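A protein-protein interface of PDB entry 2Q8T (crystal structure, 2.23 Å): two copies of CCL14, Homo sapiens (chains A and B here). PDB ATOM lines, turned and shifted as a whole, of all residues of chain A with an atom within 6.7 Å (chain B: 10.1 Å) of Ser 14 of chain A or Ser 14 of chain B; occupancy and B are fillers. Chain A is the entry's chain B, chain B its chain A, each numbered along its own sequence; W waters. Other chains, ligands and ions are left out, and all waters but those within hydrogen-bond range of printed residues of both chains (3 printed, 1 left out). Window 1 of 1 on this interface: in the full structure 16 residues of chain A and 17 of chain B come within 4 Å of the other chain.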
ATOM      1  N   TYR A  11     -21.750  12.860  27.486  1.00  0.00           N
ATOM      2  CA  TYR A  11     -22.405  11.623  26.990  1.00  0.00           C
ATOM      3  C   TYR A  11     -21.558  10.339  27.144  1.00  0.00           C
ATOM      4  O   TYR A  11     -21.809   9.336  26.477  1.00  0.00           O
ATOM      5  CB  TYR A  11     -22.931  11.835  25.569  1.00  0.00           C
ATOM      6  CG  TYR A  11     -23.522  13.208  25.429  1.00  0.00           C
ATOM      7  CD1 TYR A  11     -24.788  13.514  25.958  1.00  0.00           C
ATOM      8  CD2 TYR A  11     -22.795  14.222  24.826  1.00  0.00           C
ATOM      9  CE1 TYR A  11     -25.319  14.800  25.853  1.00  0.00           C
ATOM     10  CE2 TYR A  11     -23.308  15.487  24.723  1.00  0.00           C
ATOM     11  CZ  TYR A  11     -24.574  15.780  25.228  1.00  0.00           C
ATOM     12  OH  TYR A  11     -25.049  17.090  25.092  1.00  0.00           O
ATOM     13  N   HIS A  12     -20.607  10.363  28.093  1.00  0.00           N
ATOM     14  CA  HIS A  12     -19.711   9.239  28.316  1.00  0.00           C
ATOM     15  C   HIS A  12     -20.464   8.012  28.828  1.00  0.00           C
ATOM     16  O   HIS A  12     -21.302   8.132  29.697  1.00  0.00           O
ATOM     17  CB  HIS A  12     -18.578   9.644  29.279  1.00  0.00           C
ATOM     18  CG  HIS A  12     -17.382   8.749  29.178  1.00  0.00           C
ATOM     19  ND1 HIS A  12     -17.224   7.627  29.971  1.00  0.00           N
ATOM     20  CD2 HIS A  12     -16.307   8.782  28.356  1.00  0.00           C
ATOM     21  CE1 HIS A  12     -16.113   6.993  29.622  1.00  0.00           C
ATOM     22  NE2 HIS A  12     -15.529   7.685  28.658  1.00  0.00           N
ATOM     23  N   PRO A  13     -20.164   6.809  28.310  1.00  0.00           N
ATOM     24  CA  PRO A  13     -20.898   5.721  28.932  1.00  0.00           C
ATOM     25  C   PRO A  13     -20.505   5.473  30.402  1.00  0.00           C
ATOM     26  O   PRO A  13     -19.499   6.001  30.896  1.00  0.00           O
ATOM     27  CB  PRO A  13     -20.558   4.508  28.058  1.00  0.00           C
ATOM     28  CG  PRO A  13     -19.255   4.851  27.393  1.00  0.00           C
ATOM     29  CD  PRO A  13     -19.268   6.346  27.238  1.00  0.00           C
ATOM     30  N   SER A  14     -21.335   4.678  31.072  1.00  0.00           N
ATOM     31  CA  SER A  14     -21.138   4.262  32.466  1.00  0.00           C
ATOM     32  C   SER A  14     -20.736   2.789  32.543  1.00  0.00           C
ATOM     33  O   SER A  14     -21.209   1.968  31.780  1.00  0.00           O
ATOM     34  CB  SER A  14     -22.444   4.449  33.245  1.00  0.00           C
ATOM     35  OG  SER A  14     -22.780   5.815  33.324  1.00  0.00           O
ATOM     36  N   GLU A  15     -19.875   2.457  33.482  1.00  0.00           N
ATOM     37  CA  GLU A  15     -19.474   1.073  33.713  1.00  0.00           C
ATOM     38  C   GLU A  15     -20.493   0.333  34.605  1.00  0.00           C
ATOM     39  O   GLU A  15     -20.870   0.812  35.664  1.00  0.00           O
ATOM     40  CB  GLU A  15     -18.108   1.057  34.410  1.00  0.00           C
ATOM     41  CG  GLU A  15     -16.933   1.660  33.587  1.00  0.00           C
ATOM     42  CD  GLU A  15     -16.346   0.632  32.681  1.00  0.00           C
ATOM     43  OE1 GLU A  15     -16.885  -0.500  32.640  1.00  0.00           O
ATOM     44  OE2 GLU A  15     -15.338   0.910  32.008  1.00  0.00           O
ATOM     45  N   CYS A  16     -20.955  -0.830  34.169  1.00  0.00           N
ATOM     46  CA  CYS A  16     -21.848  -1.656  34.985  1.00  0.00           C
ATOM     47  C   CYS A  16     -21.239  -3.079  35.128  1.00  0.00           C
ATOM     48  O   CYS A  16     -20.549  -3.554  34.241  1.00  0.00           O
ATOM     49  CB  CYS A  16     -23.243  -1.757  34.306  1.00  0.00           C
ATOM     50  SG  CYS A  16     -24.046  -0.179  34.205  1.00  0.00           S
ATOM     51  N   CYS A  17     -21.619  -3.768  36.190  1.00  0.00           N
ATOM     52  CA  CYS A  17     -21.202  -5.143  36.420  1.00  0.00           C
ATOM     53  C   CYS A  17     -22.398  -6.075  36.164  1.00  0.00           C
ATOM     54  O   CYS A  17     -23.517  -5.856  36.684  1.00  0.00           O
ATOM     55  CB  CYS A  17     -20.665  -5.304  37.872  1.00  0.00           C
ATOM     56  SG  CYS A  17     -19.026  -4.523  38.054  1.00  0.00           S
ATOM     57  N   PHE A  18     -22.145  -7.122  35.403  1.00  0.00           N
ATOM     58  CA  PHE A  18     -23.194  -8.094  35.130  1.00  0.00           C
ATOM     59  C   PHE A  18     -22.896  -9.422  35.727  1.00  0.00           C
ATOM     60  O   PHE A  18     -23.791 -10.225  35.877  1.00  0.00           O
ATOM     61  CB  PHE A  18     -23.459  -8.201  33.621  1.00  0.00           C
ATOM     62  CG  PHE A  18     -24.107  -6.962  33.061  1.00  0.00           C
ATOM     63  CD1 PHE A  18     -25.373  -6.578  33.502  1.00  0.00           C
ATOM     64  CD2 PHE A  18     -23.457  -6.181  32.124  1.00  0.00           C
ATOM     65  CE1 PHE A  18     -25.994  -5.443  32.975  1.00  0.00           C
ATOM     66  CE2 PHE A  18     -24.070  -5.034  31.603  1.00  0.00           C
ATOM     67  CZ  PHE A  18     -25.329  -4.672  32.029  1.00  0.00           C
ATOM     68  N   ASN A  37     -22.255   2.862  38.605  1.00  0.00           N
ATOM     69  CA  ASN A  37     -23.349   3.804  38.557  1.00  0.00           C
ATOM     70  C   ASN A  37     -24.632   3.239  39.170  1.00  0.00           C
ATOM     71  O   ASN A  37     -24.999   2.089  38.905  1.00  0.00           O
ATOM     72  CB  ASN A  37     -23.572   4.214  37.085  1.00  0.00           C
ATOM     73  CG  ASN A  37     -24.389   5.511  36.941  1.00  0.00           C
ATOM     74  OD1 ASN A  37     -25.558   5.562  37.309  1.00  0.00           O
ATOM     75  ND2 ASN A  37     -23.768   6.549  36.404  1.00  0.00           N
ATOM     76  N   GLN A  39     -27.553   3.705  38.338  1.00  0.00           N
ATOM     77  CA  GLN A  39     -28.491   3.357  37.291  1.00  0.00           C
ATOM     78  C   GLN A  39     -28.275   1.950  36.730  1.00  0.00           C
ATOM     79  O   GLN A  39     -29.142   1.421  36.042  1.00  0.00           O
ATOM     80  CB  GLN A  39     -28.389   4.383  36.149  1.00  0.00           C
ATOM     81  CG  GLN A  39     -28.881   5.796  36.518  1.00  0.00           C
ATOM     82  CD  GLN A  39     -28.940   6.705  35.297  1.00  0.00           C
ATOM     83  OE1 GLN A  39     -29.914   6.680  34.515  1.00  0.00           O
ATOM     84  NE2 GLN A  39     -27.883   7.491  35.108  1.00  0.00           N
ATOM     85  N   CYS A  40     -27.121   1.335  36.983  1.00  0.00           N
ATOM     86  CA  CYS A  40     -26.868  -0.032  36.539  1.00  0.00           C
ATOM     87  C   CYS A  40     -27.904  -0.948  37.160  1.00  0.00           C
ATOM     88  O   CYS A  40     -28.441  -0.660  38.208  1.00  0.00           O
ATOM     89  CB  CYS A  40     -25.436  -0.472  36.931  1.00  0.00           C
ATOM     90  SG  CYS A  40     -24.070   0.455  36.180  1.00  0.00           S
ATOM     91  N   CYS A  56     -15.094  -6.925  38.449  1.00  0.00           N
ATOM     92  CA  CYS A  56     -16.425  -6.763  39.101  1.00  0.00           C
ATOM     93  C   CYS A  56     -16.601  -7.665  40.315  1.00  0.00           C
ATOM     94  O   CYS A  56     -16.274  -8.821  40.274  1.00  0.00           O
ATOM     95  CB  CYS A  56     -17.527  -7.099  38.111  1.00  0.00           C
ATOM     96  SG  CYS A  56     -17.694  -5.776  36.913  1.00  0.00           S
ATOM     97  N   PRO B  10     -18.916 -10.905  30.790  1.00  0.00           N
ATOM     98  CA  PRO B  10     -17.618 -10.272  31.133  1.00  0.00           C
ATOM     99  C   PRO B  10     -17.453 -10.107  32.646  1.00  0.00           C
ATOM    100  O   PRO B  10     -18.351  -9.574  33.318  1.00  0.00           O
ATOM    101  CB  PRO B  10     -17.701  -8.892  30.456  1.00  0.00           C
ATOM    102  CG  PRO B  10     -18.893  -8.954  29.506  1.00  0.00           C
ATOM    103  CD  PRO B  10     -19.842  -9.948  30.157  1.00  0.00           C
ATOM    104  N   TYR B  11     -16.341 -10.591  33.193  1.00  0.00           N
ATOM    105  CA  TYR B  11     -15.991 -10.318  34.624  1.00  0.00           C
ATOM    106  C   TYR B  11     -15.346  -8.912  34.891  1.00  0.00           C
ATOM    107  O   TYR B  11     -15.228  -8.441  36.008  1.00  0.00           O
ATOM    108  CB  TYR B  11     -15.140 -11.414  35.118  1.00  0.00           C
ATOM    109  CG  TYR B  11     -15.871 -12.656  35.652  1.00  0.00           C
ATOM    110  CD1 TYR B  11     -16.142 -12.779  37.014  1.00  0.00           C
ATOM    111  CD2 TYR B  11     -16.186 -13.759  34.806  1.00  0.00           C
ATOM    112  CE1 TYR B  11     -16.733 -13.952  37.547  1.00  0.00           C
ATOM    113  CE2 TYR B  11     -16.789 -14.964  35.345  1.00  0.00           C
ATOM    114  CZ  TYR B  11     -17.056 -15.033  36.732  1.00  0.00           C
ATOM    115  OH  TYR B  11     -17.624 -16.184  37.347  1.00  0.00           O
ATOM    116  N   HIS B  12     -14.964  -8.269  33.808  1.00  0.00           N
ATOM    117  CA  HIS B  12     -14.651  -6.903  33.812  1.00  0.00           C
ATOM    118  C   HIS B  12     -15.950  -6.132  33.606  1.00  0.00           C
ATOM    119  O   HIS B  12     -16.930  -6.703  33.200  1.00  0.00           O
ATOM    120  CB  HIS B  12     -13.641  -6.612  32.720  1.00  0.00           C
ATOM    121  CG  HIS B  12     -14.069  -7.025  31.358  1.00  0.00           C
ATOM    122  ND1 HIS B  12     -14.832  -6.219  30.544  1.00  0.00           N
ATOM    123  CD2 HIS B  12     -13.757  -8.118  30.617  1.00  0.00           C
ATOM    124  CE1 HIS B  12     -14.988  -6.801  29.366  1.00  0.00           C
ATOM    125  NE2 HIS B  12     -14.342  -7.948  29.381  1.00  0.00           N
ATOM    126  N   PRO B  13     -15.984  -4.869  33.977  1.00  0.00           N
ATOM    127  CA  PRO B  13     -17.232  -4.202  33.761  1.00  0.00           C
ATOM    128  C   PRO B  13     -17.506  -3.954  32.266  1.00  0.00           C
ATOM    129  O   PRO B  13     -16.540  -3.941  31.440  1.00  0.00           O
ATOM    130  CB  PRO B  13     -16.998  -2.871  34.451  1.00  0.00           C
ATOM    131  CG  PRO B  13     -15.514  -2.626  34.296  1.00  0.00           C
ATOM    132  CD  PRO B  13     -14.988  -3.967  34.613  1.00  0.00           C
ATOM    133  N   SER B  14     -18.800  -3.717  31.953  1.00  0.00           N
ATOM    134  CA  SER B  14     -19.256  -3.366  30.613  1.00  0.00           C
ATOM    135  C   SER B  14     -19.862  -1.954  30.574  1.00  0.00           C
ATOM    136  O   SER B  14     -20.351  -1.500  31.568  1.00  0.00           O
ATOM    137  CB  SER B  14     -20.269  -4.406  30.120  1.00  0.00           C
ATOM    138  OG  SER B  14     -20.090  -5.655  30.808  1.00  0.00           O
ATOM    139  N   GLU B  15     -19.779  -1.279  29.427  1.00  0.00           N
ATOM    140  CA  GLU B  15     -20.346   0.057  29.169  1.00  0.00           C
ATOM    141  C   GLU B  15     -21.840   0.003  28.863  1.00  0.00           C
ATOM    142  O   GLU B  15     -22.264  -0.836  28.056  1.00  0.00           O
ATOM    143  CB  GLU B  15     -19.731   0.700  27.926  1.00  0.00           C
ATOM    144  CG  GLU B  15     -18.346   1.169  28.101  1.00  0.00           C
ATOM    145  CD  GLU B  15     -17.379  -0.002  28.144  1.00  0.00           C
ATOM    146  OE1 GLU B  15     -17.690  -1.093  27.570  1.00  0.00           O
ATOM    147  OE2 GLU B  15     -16.317   0.179  28.780  1.00  0.00           O
ATOM    148  N   CYS B  16     -22.613   0.900  29.498  1.00  0.00           N
ATOM    149  CA  CYS B  16     -24.015   1.115  29.162  1.00  0.00           C
ATOM    150  C   CYS B  16     -24.220   2.605  29.043  1.00  0.00           C
ATOM    151  O   CYS B  16     -23.530   3.392  29.680  1.00  0.00           O
ATOM    152  CB  CYS B  16     -24.973   0.564  30.263  1.00  0.00           C
ATOM    153  SG  CYS B  16     -24.789  -1.207  30.607  1.00  0.00           S
ATOM    154  N   CYS B  17     -25.244   2.970  28.308  1.00  0.00           N
ATOM    155  CA  CYS B  17     -25.613   4.361  28.066  1.00  0.00           C
ATOM    156  C   CYS B  17     -26.930   4.605  28.803  1.00  0.00           C
ATOM    157  O   CYS B  17     -27.897   3.870  28.605  1.00  0.00           O
ATOM    158  CB  CYS B  17     -25.805   4.525  26.538  1.00  0.00           C
ATOM    159  SG  CYS B  17     -24.209   4.445  25.652  1.00  0.00           S
ATOM    160  N   PHE B  18     -26.947   5.613  29.667  1.00  0.00           N
ATOM    161  CA  PHE B  18     -28.156   6.006  30.429  1.00  0.00           C
ATOM    162  C   PHE B  18     -28.721   7.300  29.899  1.00  0.00           C
ATOM    163  O   PHE B  18     -29.877   7.613  30.140  1.00  0.00           O
ATOM    164  CB  PHE B  18     -27.848   6.099  31.921  1.00  0.00           C
ATOM    165  CG  PHE B  18     -27.414   4.764  32.511  1.00  0.00           C
ATOM    166  CD1 PHE B  18     -28.262   3.663  32.436  1.00  0.00           C
ATOM    167  CD2 PHE B  18     -26.158   4.610  33.064  1.00  0.00           C
ATOM    168  CE1 PHE B  18     -27.870   2.439  32.926  1.00  0.00           C
ATOM    169  CE2 PHE B  18     -25.762   3.377  33.562  1.00  0.00           C
ATOM    170  CZ  PHE B  18     -26.595   2.307  33.498  1.00  0.00           C
ATOM    171  N   THR B  19     -27.902   8.016  29.138  1.00  0.00           N
ATOM    172  CA  THR B  19     -28.322   9.195  28.429  1.00  0.00           C
ATOM    173  C   THR B  19     -27.732   9.207  27.000  1.00  0.00           C
ATOM    174  O   THR B  19     -26.611   8.763  26.801  1.00  0.00           O
ATOM    175  CB  THR B  19     -27.955  10.480  29.224  1.00  0.00           C
ATOM    176  OG1 THR B  19     -28.649  11.572  28.652  1.00  0.00           O
ATOM    177  CG2 THR B  19     -26.550  10.799  29.127  1.00  0.00           C
ATOM    178  N   TYR B  20     -28.501   9.651  26.006  1.00  0.00           N
ATOM    179  CA  TYR B  20     -27.966   9.878  24.663  1.00  0.00           C
ATOM    180  C   TYR B  20     -27.710  11.376  24.353  1.00  0.00           C
ATOM    181  O   TYR B  20     -28.383  12.276  24.887  1.00  0.00           O
ATOM    182  CB  TYR B  20     -28.938   9.351  23.621  1.00  0.00           C
ATOM    183  CG  TYR B  20     -29.439   7.935  23.816  1.00  0.00           C
ATOM    184  CD1 TYR B  20     -28.543   6.853  23.842  1.00  0.00           C
ATOM    185  CD2 TYR B  20     -30.837   7.666  23.919  1.00  0.00           C
ATOM    186  CE1 TYR B  20     -28.992   5.509  24.001  1.00  0.00           C
ATOM    187  CE2 TYR B  20     -31.308   6.334  24.069  1.00  0.00           C
ATOM    188  CZ  TYR B  20     -30.358   5.268  24.097  1.00  0.00           C
ATOM    189  OH  TYR B  20     -30.774   3.989  24.228  1.00  0.00           O
ATOM    190  N   TYR B  34     -18.707   1.266  18.968  1.00  0.00           N
ATOM    191  CA  TYR B  34     -19.144  -0.092  19.363  1.00  0.00           C
ATOM    192  C   TYR B  34     -20.559  -0.001  19.965  1.00  0.00           C
ATOM    193  O   TYR B  34     -21.043   1.068  20.307  1.00  0.00           O
ATOM    194  CB  TYR B  34     -18.153  -0.728  20.339  1.00  0.00           C
ATOM    195  CG  TYR B  34     -17.999   0.117  21.633  1.00  0.00           C
ATOM    196  CD1 TYR B  34     -18.921   0.001  22.686  1.00  0.00           C
ATOM    197  CD2 TYR B  34     -16.968   1.021  21.780  1.00  0.00           C
ATOM    198  CE1 TYR B  34     -18.793   0.759  23.850  1.00  0.00           C
ATOM    199  CE2 TYR B  34     -16.812   1.775  22.939  1.00  0.00           C
ATOM    200  CZ  TYR B  34     -17.747   1.625  23.975  1.00  0.00           C
ATOM    201  OH  TYR B  34     -17.650   2.398  25.127  1.00  0.00           O
ATOM    202  N   GLU B  35     -21.226  -1.145  20.035  1.00  0.00           N
ATOM    203  CA  GLU B  35     -22.544  -1.287  20.645  1.00  0.00           C
ATOM    204  C   GLU B  35     -22.313  -1.655  22.092  1.00  0.00           C
ATOM    205  O   GLU B  35     -21.416  -2.399  22.423  1.00  0.00           O
ATOM    206  CB  GLU B  35     -23.349  -2.415  19.936  1.00  0.00           C
ATOM    207  CG  GLU B  35     -23.186  -2.349  18.443  1.00  0.00           C
ATOM    208  CD  GLU B  35     -24.080  -3.303  17.696  1.00  0.00           C
ATOM    209  OE1 GLU B  35     -24.641  -4.235  18.349  1.00  0.00           O
ATOM    210  OE2 GLU B  35     -24.223  -3.106  16.445  1.00  0.00           O
ATOM    211  N   THR B  36     -23.101  -1.084  22.975  1.00  0.00           N
ATOM    212  CA  THR B  36     -23.070  -1.485  24.349  1.00  0.00           C
ATOM    213  C   THR B  36     -23.503  -2.948  24.546  1.00  0.00           C
ATOM    214  O   THR B  36     -24.146  -3.586  23.693  1.00  0.00           O
ATOM    215  CB  THR B  36     -23.976  -0.587  25.201  1.00  0.00           C
ATOM    216  OG1 THR B  36     -25.318  -0.640  24.679  1.00  0.00           O
ATOM    217  CG2 THR B  36     -23.448   0.803  25.180  1.00  0.00           C
ATOM    218  N   ASN B  37     -23.154  -3.464  25.713  1.00  0.00           N
ATOM    219  CA  ASN B  37     -23.494  -4.834  26.083  1.00  0.00           C
ATOM    220  C   ASN B  37     -25.002  -5.089  25.964  1.00  0.00           C
ATOM    221  O   ASN B  37     -25.803  -4.255  26.402  1.00  0.00           O
ATOM    222  CB  ASN B  37     -22.980  -5.106  27.497  1.00  0.00           C
ATOM    223  CG  ASN B  37     -22.847  -6.580  27.775  1.00  0.00           C
ATOM    224  OD1 ASN B  37     -23.838  -7.265  27.983  1.00  0.00           O
ATOM    225  ND2 ASN B  37     -21.619  -7.079  27.764  1.00  0.00           N
ATOM    226  N   SER B  38     -25.386  -6.228  25.361  1.00  0.00           N
ATOM    227  CA  SER B  38     -26.793  -6.658  25.299  1.00  0.00           C
ATOM    228  C   SER B  38     -27.476  -6.697  26.676  1.00  0.00           C
ATOM    229  O   SER B  38     -28.688  -6.557  26.740  1.00  0.00           O
ATOM    230  CB  SER B  38     -26.902  -8.082  24.753  1.00  0.00           C
ATOM    231  OG  SER B  38     -25.615  -8.604  24.422  1.00  0.00           O
ATOM    232  N   GLN B  39     -26.716  -6.906  27.769  1.00  0.00           N
ATOM    233  CA  GLN B  39     -27.325  -6.995  29.104  1.00  0.00           C
ATOM    234  C   GLN B  39     -27.722  -5.606  29.615  1.00  0.00           C
ATOM    235  O   GLN B  39     -28.440  -5.486  30.625  1.00  0.00           O
ATOM    236  CB  GLN B  39     -26.409  -7.715  30.107  1.00  0.00           C
ATOM    237  CG  GLN B  39     -25.834  -9.087  29.606  1.00  0.00           C
ATOM    238  CD  GLN B  39     -24.973  -9.817  30.645  1.00  0.00           C
ATOM    239  OE1 GLN B  39     -25.483 -10.371  31.621  1.00  0.00           O
ATOM    240  NE2 GLN B  39     -23.669  -9.836  30.417  1.00  0.00           N
ATOM    241  N   CYS B  40     -27.248  -4.556  28.935  1.00  0.00           N
ATOM    242  CA  CYS B  40     -27.640  -3.150  29.283  1.00  0.00           C
ATOM    243  C   CYS B  40     -29.159  -2.953  29.154  1.00  0.00           C
ATOM    244  O   CYS B  40     -29.792  -3.630  28.371  1.00  0.00           O
ATOM    245  CB  CYS B  40     -26.883  -2.099  28.447  1.00  0.00           C
ATOM    246  SG  CYS B  40     -25.046  -2.075  28.732  1.00  0.00           S
ATOM    247  N   SER B  41     -29.731  -2.030  29.912  1.00  0.00           N
ATOM    248  CA  SER B  41     -31.181  -1.900  29.951  1.00  0.00           C
ATOM    249  C   SER B  41     -31.726  -1.289  28.645  1.00  0.00           C
ATOM    250  O   SER B  41     -32.822  -1.668  28.169  1.00  0.00           O
ATOM    251  CB  SER B  41     -31.630  -1.092  31.167  1.00  0.00           C
ATOM    252  OG  SER B  41     -31.029   0.187  31.175  1.00  0.00           O
ATOM    253  N   LYS B  42     -30.958  -0.346  28.096  1.00  0.00           N
ATOM    254  CA  LYS B  42     -31.213   0.213  26.774  1.00  0.00           C
ATOM    255  C   LYS B  42     -30.002   0.041  25.890  1.00  0.00           C
ATOM    256  O   LYS B  42     -28.869   0.068  26.376  1.00  0.00           O
ATOM    257  CB  LYS B  42     -31.631   1.688  26.828  1.00  0.00           C
ATOM    258  CG  LYS B  42     -31.387   2.371  28.176  1.00  0.00           C
ATOM    259  CD  LYS B  42     -30.997   3.842  28.034  1.00  0.00           C
ATOM    260  CE  LYS B  42     -32.199   4.755  28.024  1.00  0.00           C
ATOM    261  NZ  LYS B  42     -31.669   6.134  27.850  1.00  0.00           N
ATOM    262  N   GLY B  44     -27.209   1.010  23.022  1.00  0.00           N
ATOM    263  CA  GLY B  44     -26.490   2.245  22.813  1.00  0.00           C
ATOM    264  C   GLY B  44     -25.442   1.973  21.769  1.00  0.00           C
ATOM    265  O   GLY B  44     -24.963   0.859  21.627  1.00  0.00           O
ATOM    266  N   VAL B  46     -21.877   3.551  20.980  1.00  0.00           N
ATOM    267  CA  VAL B  46     -20.868   4.446  21.466  1.00  0.00           C
ATOM    268  C   VAL B  46     -19.921   4.830  20.338  1.00  0.00           C
ATOM    269  O   VAL B  46     -19.255   3.972  19.830  1.00  0.00           O
ATOM    270  CB  VAL B  46     -20.064   3.823  22.622  1.00  0.00           C
ATOM    271  CG1 VAL B  46     -19.007   4.887  23.181  1.00  0.00           C
ATOM    272  CG2 VAL B  46     -21.010   3.353  23.701  1.00  0.00           C
ATOM    273  N   SER B  54     -15.777   9.329  24.137  1.00  0.00           N
ATOM    274  CA  SER B  54     -16.784   8.282  23.930  1.00  0.00           C
ATOM    275  C   SER B  54     -18.113   8.944  24.098  1.00  0.00           C
ATOM    276  O   SER B  54     -18.348   9.602  25.108  1.00  0.00           O
ATOM    277  CB  SER B  54     -16.679   7.145  24.992  1.00  0.00           C
ATOM    278  OG  SER B  54     -15.449   6.482  24.870  1.00  0.00           O
ATOM    279  N   VAL B  55     -18.988   8.771  23.107  1.00  0.00           N
ATOM    280  CA  VAL B  55     -20.240   9.508  23.051  1.00  0.00           C
ATOM    281  C   VAL B  55     -21.390   8.528  22.835  1.00  0.00           C
ATOM    282  O   VAL B  55     -21.486   7.897  21.776  1.00  0.00           O
ATOM    283  CB  VAL B  55     -20.242  10.526  21.873  1.00  0.00           C
ATOM    284  CG1 VAL B  55     -21.558  11.285  21.836  1.00  0.00           C
ATOM    285  CG2 VAL B  55     -18.983  11.537  21.943  1.00  0.00           C
ATOM    286  N   CYS B  56     -22.278   8.437  23.813  1.00  0.00           N
ATOM    287  CA  CYS B  56     -23.484   7.590  23.770  1.00  0.00           C
ATOM    288  C   CYS B  56     -24.523   8.189  22.838  1.00  0.00           C
ATOM    289  O   CYS B  56     -24.837   9.374  22.953  1.00  0.00           O
ATOM    290  CB  CYS B  56     -24.128   7.489  25.183  1.00  0.00           C
ATOM    291  SG  CYS B  56     -23.280   6.280  26.185  1.00  0.00           S
HETATM  292  O   HOH W   1     -18.823  12.504  25.730  1.00  0.00           O
HETATM  293  O   HOH W   2     -19.761  -7.292  33.469  1.00  0.00           O
HETATM  294  O   HOH W   3     -30.072  -0.190  34.104  1.00  0.00           O
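The side-chain sulfur (SG) of Cys 17 of chain B forms a disulfide with the side-chain sulfur (SG) of Cys 56 of chain B (2.1 Å).
OD1 of Asn 37 of chain B lies within hydrogen-bond range of N of Gln 39 of chain B (2.9 Å).
N of Gln 39 of chain A lies within hydrogen-bond range of OD1 of Asn 37 of chain A.
Water W2 lies within hydrogen-bond range of O of Pro 10 of chain B (2.7 Å), O of His 12 of chain B (2.9 Å), N of Phe 18 of chain A (3.1 Å) and OG of Ser 14 of chain B (3.1 Å).
Water W1 lies within hydrogen-bond range of O of Ser 54 of chain B (3.0 Å) and N of Tyr 11 of chain A (3.4 Å).
Of the 12 printed residues of chain A, 10 touch a printed residue of chain B.
Printed residues of chain A that touch a printed residue of chain B: Tyr 11, His 12, Pro 13, Ser 14, Glu 15, Cys 16, Phe 18, Gln 39, Cys 40 and Cys 56.
Along chain B the printed residues that touch a printed residue of chain A span positions 11 to 56.
Among the printed residues, no Asp or Glu carboxylate lies within 4 Å of a Lys or Arg side-chain nitrogen of the other chain.
The backbone NH (N) of Cys 56 of chain A sits at hydrogen-bond distance from the backbone carbonyl oxygen (O) of Tyr 11 of chain B (2.9 Å).
The backbone NH of Cys 16 of chain A sits at hydrogen-bond distance from the backbone carbonyl oxygen of Ser 14 of chain B, at 2.8 Å.
The backbone NH (N) of Cys 16 of chain B sits at hydrogen-bond distance from the backbone carbonyl oxygen (O) of Ser 14 of chain A, at 2.9 Å.
The backbone NH of Cys 56 of chain B is in hydrogen-bond range of the backbone carbonyl oxygen of Tyr 11 of chain A, 2.9 Å away.
The side-chain carboxylate of Glu 15 of chain B sits close to the side-chain carboxylate of Glu 15 of chain A (3.5 Å).
SG of Cys 56 of chain A lies close to N of Pro 13 of chain B, 3.5 Å away.
Tyr 11 of chain A touches Cys 56 of chain B, and with the chains exchanged Cys 56 of chain A touches Tyr 11 of chain B.
Cys 56 of chain A touches His 12 of chain B, but with the chains exchanged His 12 of chain A does not touch Cys 56 of chain B (4.2 Å).
Of chain B, only Ser 14 (3.6 Å), Glu 15 (3.3 Å), Cys 16 (2.9 Å) and Phe 18 (3.5 Å) come within 4 Å of Ser 14 of chain A.
Ser 14 of chain B touches four residues of chain A.
Glu 15 of chain A touches just these residues of chain B: Pro 13, Ser 14 and Glu 15.
Cys 16 of chain A touches just these residues of chain B: Pro 13, Ser 14, Cys 16 and Phe 18.
Printed residues of chain A within 4 Å of Glu 15 of chain B: Pro 13, Ser 14 and Glu 15.
Of the printed residues of chain A, Cys 16 of chain B touches Pro 13, Ser 14, Cys 16 and Phe 18.
Printed residues of chain A within 4 Å of His 12 of chain B: Cys 56 (3.8 Å).
The nearest residue of chain A that does not touch Ser 14 of chain B is Cys 17 of chain A (5.1 Å).
The nearest printed residue of chain B that does not touch Cys 40 of chain A is Cys 16 of chain B (5.9 Å).
Among the printed residues, merely in contact across the chains: Tyr 11 of chain A with Tyr 20 of chain B (3.95 Å), Tyr 11 of chain A with Ser 54 of chain B (3.7 Å), Tyr 11 of chain A with Val 55 of chain B (3.8 Å), His 12 of chain A with Ser 54 of chain B (3.5 Å), Pro 13 of chain A with Glu 15 of chain B (3.9 Å), Pro 13 of chain A with Cys 16 of chain B (3.6 Å), Pro 13 of chain A with Tyr 34 of chain B (3.7 Å), Pro 13 of chain A with Ser 54 of chain B (3.5 Å), Pro 13 of chain A with Cys 56 of chain B (3.7 Å), Ser 14 of chain A with Ser 14 of chain B (3.6 Å), Ser 14 of chain A with Glu 15 of chain B (3.3 Å), Ser 14 of chain A with Phe 18 of chain B (3.5 Å), Glu 15 of chain A with Pro 13 of chain B (3.0 Å), Glu 15 of chain A with Ser 14 of chain B (3.5 Å), Cys 16 of chain A with Pro 13 of chain B (3.4 Å), Cys 16 of chain A with Cys 16 of chain B (3.8 Å), Cys 16 of chain A with Phe 18 of chain B (3.6 Å), Phe 18 of chain A with Ser 14 of chain B (3.7 Å), Phe 18 of chain A with Cys 16 of chain B (3.8 Å), Phe 18 of chain A with Gln 39 of chain B (3.4 Å), Phe 18 of chain A with Cys 40 of chain B (3.6 Å), Gln 39 of chain A with Phe 18 of chain B (3.4 Å), Cys 40 of chain A with Phe 18 of chain B (3.7 Å) and Cys 56 of chain A with His 12 of chain B (3.8 Å).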
